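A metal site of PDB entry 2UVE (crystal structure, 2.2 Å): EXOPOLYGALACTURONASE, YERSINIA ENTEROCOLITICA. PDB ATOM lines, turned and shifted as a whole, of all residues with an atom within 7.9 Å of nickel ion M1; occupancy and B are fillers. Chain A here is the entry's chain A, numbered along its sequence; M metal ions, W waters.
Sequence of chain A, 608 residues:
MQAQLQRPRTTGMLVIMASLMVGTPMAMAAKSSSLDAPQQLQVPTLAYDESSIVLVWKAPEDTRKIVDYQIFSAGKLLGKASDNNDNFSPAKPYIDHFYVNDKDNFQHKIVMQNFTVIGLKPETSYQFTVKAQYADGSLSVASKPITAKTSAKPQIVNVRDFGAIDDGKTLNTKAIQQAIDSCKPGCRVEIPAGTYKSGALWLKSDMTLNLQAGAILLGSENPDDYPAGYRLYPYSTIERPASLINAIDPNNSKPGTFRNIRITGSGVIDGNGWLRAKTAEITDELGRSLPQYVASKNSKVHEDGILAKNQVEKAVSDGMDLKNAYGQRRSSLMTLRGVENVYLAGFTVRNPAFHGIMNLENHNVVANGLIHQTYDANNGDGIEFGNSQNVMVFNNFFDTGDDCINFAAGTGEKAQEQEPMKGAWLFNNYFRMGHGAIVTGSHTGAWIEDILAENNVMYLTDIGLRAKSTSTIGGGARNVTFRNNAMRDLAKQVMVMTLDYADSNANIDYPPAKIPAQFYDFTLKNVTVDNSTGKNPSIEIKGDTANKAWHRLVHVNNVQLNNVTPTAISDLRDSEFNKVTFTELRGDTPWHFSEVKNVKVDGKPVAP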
ATOM      1  N   ALA A 295      29.723 -20.596 -23.419  1.00  0.00           N
ATOM      2  CA  ALA A 295      28.588 -21.020 -24.284  1.00  0.00           C
ATOM      3  C   ALA A 295      28.655 -20.261 -25.616  1.00  0.00           C
ATOM      4  O   ALA A 295      28.359 -19.079 -25.692  1.00  0.00           O
ATOM      5  CB  ALA A 295      27.218 -20.819 -23.597  1.00  0.00           C
ATOM      6  N   THR A 374      31.601 -30.263 -18.363  1.00  0.00           N
ATOM      7  CA  THR A 374      31.646 -29.668 -19.719  1.00  0.00           C
ATOM      8  C   THR A 374      30.680 -28.527 -19.940  1.00  0.00           C
ATOM      9  O   THR A 374      30.617 -28.001 -21.024  1.00  0.00           O
ATOM     10  CB  THR A 374      31.502 -30.711 -20.836  1.00  0.00           C
ATOM     11  OG1 THR A 374      30.161 -31.212 -20.917  1.00  0.00           O
ATOM     12  CG2 THR A 374      32.472 -31.853 -20.633  1.00  0.00           C
ATOM     13  N   TYR A 375      29.992 -28.096 -18.901  1.00  0.00           N
ATOM     14  CA  TYR A 375      29.173 -26.852 -18.943  1.00  0.00           C
ATOM     15  C   TYR A 375      30.056 -25.608 -19.252  1.00  0.00           C
ATOM     16  O   TYR A 375      31.095 -25.442 -18.624  1.00  0.00           O
ATOM     17  CB  TYR A 375      28.446 -26.650 -17.611  1.00  0.00           C
ATOM     18  CG  TYR A 375      27.466 -25.534 -17.651  1.00  0.00           C
ATOM     19  CD1 TYR A 375      26.194 -25.695 -18.224  1.00  0.00           C
ATOM     20  CD2 TYR A 375      27.810 -24.282 -17.146  1.00  0.00           C
ATOM     21  CE1 TYR A 375      25.294 -24.633 -18.284  1.00  0.00           C
ATOM     22  CE2 TYR A 375      26.938 -23.218 -17.200  1.00  0.00           C
ATOM     23  CZ  TYR A 375      25.687 -23.386 -17.767  1.00  0.00           C
ATOM     24  OH  TYR A 375      24.859 -22.284 -17.800  1.00  0.00           O
ATOM     25  N   ASP A 376      29.684 -24.754 -20.219  1.00  0.00           N
ATOM     26  CA  ASP A 376      28.530 -24.939 -21.113  1.00  0.00           C
ATOM     27  C   ASP A 376      29.070 -25.017 -22.565  1.00  0.00           C
ATOM     28  O   ASP A 376      28.710 -24.216 -23.395  1.00  0.00           O
ATOM     29  CB  ASP A 376      27.544 -23.755 -20.938  1.00  0.00           C
ATOM     30  CG  ASP A 376      26.189 -24.061 -21.500  1.00  0.00           C
ATOM     31  OD1 ASP A 376      25.298 -23.182 -21.556  1.00  0.00           O
ATOM     32  OD2 ASP A 376      25.998 -25.212 -21.906  1.00  0.00           O
ATOM     33  N   ALA A 377      30.001 -25.930 -22.838  1.00  0.00           N
ATOM     34  CA  ALA A 377      30.509 -26.186 -24.214  1.00  0.00           C
ATOM     35  C   ALA A 377      29.363 -26.591 -25.185  1.00  0.00           C
ATOM     36  O   ALA A 377      28.636 -27.603 -24.964  1.00  0.00           O
ATOM     37  CB  ALA A 377      31.572 -27.305 -24.184  1.00  0.00           C
ATOM     38  N   ASN A 378      29.210 -25.779 -26.232  1.00  0.00           N
ATOM     39  CA  ASN A 378      28.173 -25.953 -27.220  1.00  0.00           C
ATOM     40  C   ASN A 378      28.282 -27.329 -27.879  1.00  0.00           C
ATOM     41  O   ASN A 378      29.327 -27.677 -28.429  1.00  0.00           O
ATOM     42  CB  ASN A 378      28.199 -24.828 -28.256  1.00  0.00           C
ATOM     43  CG  ASN A 378      26.861 -24.692 -29.003  1.00  0.00           C
ATOM     44  OD1 ASN A 378      25.816 -25.218 -28.598  1.00  0.00           O
ATOM     45  ND2 ASN A 378      26.886 -23.950 -30.077  1.00  0.00           N
ATOM     46  N   ASN A 379      27.178 -28.077 -27.775  1.00  0.00           N
ATOM     47  CA  ASN A 379      27.028 -29.501 -28.147  1.00  0.00           C
ATOM     48  C   ASN A 379      27.836 -30.509 -27.317  1.00  0.00           C
ATOM     49  O   ASN A 379      28.015 -31.677 -27.713  1.00  0.00           O
ATOM     50  CB  ASN A 379      27.182 -29.698 -29.663  1.00  0.00           C
ATOM     51  CG  ASN A 379      26.405 -28.617 -30.456  1.00  0.00           C
ATOM     52  OD1 ASN A 379      26.996 -27.675 -30.999  1.00  0.00           O
ATOM     53  ND2 ASN A 379      25.080 -28.689 -30.393  1.00  0.00           N
ATOM     54  N   GLY A 380      28.319 -30.072 -26.150  1.00  0.00           N
ATOM     55  CA  GLY A 380      29.134 -30.952 -25.319  1.00  0.00           C
ATOM     56  C   GLY A 380      28.214 -31.817 -24.467  1.00  0.00           C
ATOM     57  O   GLY A 380      28.067 -31.577 -23.249  1.00  0.00           O
ATOM     58  N   THR A 400      26.891 -30.817 -17.850  1.00  0.00           N
ATOM     59  CA  THR A 400      27.226 -30.876 -19.302  1.00  0.00           C
ATOM     60  C   THR A 400      26.809 -29.631 -20.079  1.00  0.00           C
ATOM     61  O   THR A 400      25.858 -28.908 -19.716  1.00  0.00           O
ATOM     62  CB  THR A 400      26.701 -32.196 -19.944  1.00  0.00           C
ATOM     63  OG1 THR A 400      25.288 -32.290 -19.728  1.00  0.00           O
ATOM     64  CG2 THR A 400      27.349 -33.455 -19.305  1.00  0.00           C
ATOM     65  N   GLY A 401      27.538 -29.360 -21.158  1.00  0.00           N
ATOM     66  CA  GLY A 401      27.144 -28.256 -21.999  1.00  0.00           C
ATOM     67  C   GLY A 401      25.906 -28.542 -22.830  1.00  0.00           C
ATOM     68  O   GLY A 401      25.275 -27.604 -23.297  1.00  0.00           O
ATOM     69  N   ASP A 402      25.553 -29.809 -23.028  1.00  0.00           N
ATOM     70  CA  ASP A 402      24.336 -30.184 -23.781  1.00  0.00           C
ATOM     71  C   ASP A 402      23.586 -31.263 -23.008  1.00  0.00           C
ATOM     72  O   ASP A 402      23.551 -31.237 -21.760  1.00  0.00           O
ATOM     73  CB  ASP A 402      24.697 -30.618 -25.232  1.00  0.00           C
ATOM     74  CG  ASP A 402      23.572 -30.358 -26.247  1.00  0.00           C
ATOM     75  OD1 ASP A 402      22.629 -31.167 -26.339  1.00  0.00           O
ATOM     76  OD2 ASP A 402      23.602 -29.310 -26.931  1.00  0.00           O
ATOM     77  N   ASP A 403      22.982 -32.219 -23.705  1.00  0.00           N
ATOM     78  CA  ASP A 403      22.279 -33.347 -23.023  1.00  0.00           C
ATOM     79  C   ASP A 403      23.234 -34.128 -22.158  1.00  0.00           C
ATOM     80  O   ASP A 403      24.400 -34.303 -22.556  1.00  0.00           O
ATOM     81  CB  ASP A 403      21.699 -34.323 -24.043  1.00  0.00           C
ATOM     82  CG  ASP A 403      20.730 -33.658 -25.003  1.00  0.00           C
ATOM     83  OD1 ASP A 403      20.094 -32.645 -24.646  1.00  0.00           O
ATOM     84  OD2 ASP A 403      20.569 -34.192 -26.098  1.00  0.00           O
ATOM     85  N   MET A 433      23.810 -29.777 -14.146  1.00  0.00           N
ATOM     86  CA  MET A 433      23.328 -28.981 -15.275  1.00  0.00           C
ATOM     87  C   MET A 433      23.431 -29.824 -16.518  1.00  0.00           C
ATOM     88  O   MET A 433      24.270 -30.723 -16.598  1.00  0.00           O
ATOM     89  CB  MET A 433      24.104 -27.681 -15.404  1.00  0.00           C
ATOM     90  CG  MET A 433      23.859 -26.745 -14.197  1.00  0.00           C
ATOM     91  SD  MET A 433      24.381 -25.086 -14.518  1.00  0.00           S
ATOM     92  CE  MET A 433      23.079 -24.489 -15.622  1.00  0.00           C
ATOM     93  N   GLY A 434      22.535 -29.546 -17.486  1.00  0.00           N
ATOM     94  CA  GLY A 434      22.549 -30.239 -18.753  1.00  0.00           C
ATOM     95  C   GLY A 434      21.211 -30.038 -19.429  1.00  0.00           C
ATOM     96  O   GLY A 434      20.297 -29.583 -18.775  1.00  0.00           O
ATOM     97  N   HIS A 435      21.071 -30.362 -20.707  1.00  0.00           N
ATOM     98  CA  HIS A 435      19.825 -30.045 -21.423  1.00  0.00           C
ATOM     99  C   HIS A 435      18.711 -31.073 -21.164  1.00  0.00           C
ATOM    100  O   HIS A 435      17.568 -30.842 -21.513  1.00  0.00           O
ATOM    101  CB  HIS A 435      20.096 -29.889 -22.924  1.00  0.00           C
ATOM    102  CG  HIS A 435      20.919 -28.698 -23.247  1.00  0.00           C
ATOM    103  ND1 HIS A 435      21.116 -28.250 -24.542  1.00  0.00           N
ATOM    104  CD2 HIS A 435      21.566 -27.830 -22.446  1.00  0.00           C
ATOM    105  CE1 HIS A 435      21.880 -27.174 -24.518  1.00  0.00           C
ATOM    106  NE2 HIS A 435      22.168 -26.907 -23.264  1.00  0.00           N
ATOM    107  N   ASP A 462      18.029 -29.192 -16.953  1.00  0.00           N
ATOM    108  CA  ASP A 462      16.909 -28.556 -17.651  1.00  0.00           C
ATOM    109  C   ASP A 462      15.608 -29.370 -17.565  1.00  0.00           C
ATOM    110  O   ASP A 462      14.544 -28.831 -17.269  1.00  0.00           O
ATOM    111  CB  ASP A 462      17.246 -28.319 -19.116  1.00  0.00           C
ATOM    112  CG  ASP A 462      18.094 -27.089 -19.341  1.00  0.00           C
ATOM    113  OD1 ASP A 462      18.581 -26.417 -18.412  1.00  0.00           O
ATOM    114  OD2 ASP A 462      18.255 -26.796 -20.520  1.00  0.00           O
HETATM  115 NI    NI M   1      24.167 -26.014 -22.477  1.00  0.00          NI
HETATM  116 NI    NI M   2      20.227 -28.903 -28.580  1.00  0.00          NI
HETATM  117  O   HOH W   1      24.130 -27.182 -20.422  1.00  0.00           O
HETATM  118  O   HOH W   2      24.325 -25.024 -24.458  1.00  0.00           O
HETATM  119  O   HOH W   3      22.998 -24.281 -21.766  1.00  0.00           O
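N of Gly 401 sits at hydrogen-bond distance from O of Gly 380, 3.1 Å away. The side-chain hydroxyl (OG1) of Thr 374 sits at hydrogen-bond distance from the backbone NH (N) of Gly 401, 3.2 Å away. The backbone NH of His 435 lies within hydrogen-bond range of the backbone carbonyl oxygen of Asp 402 (2.8 Å).
Three residues have an atom within 4 Å of nickel ion M1: Asp 376, Gly 401 and His 435. The nearest printed residue that does not touch nickel ion M1 is Asp 402 (4.1 Å).
Nickel ion M1 is bound by the side-chain carboxylate (OD2) of Asp 376 (2.1 Å), the backbone carbonyl oxygen (O) of Gly 401 (2.1 Å), water W3 (2.2 Å), water W2 (2.2 Å), a ring nitrogen (NE2) of His 435 (2.3 Å) and water W1 (2.4 Å).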
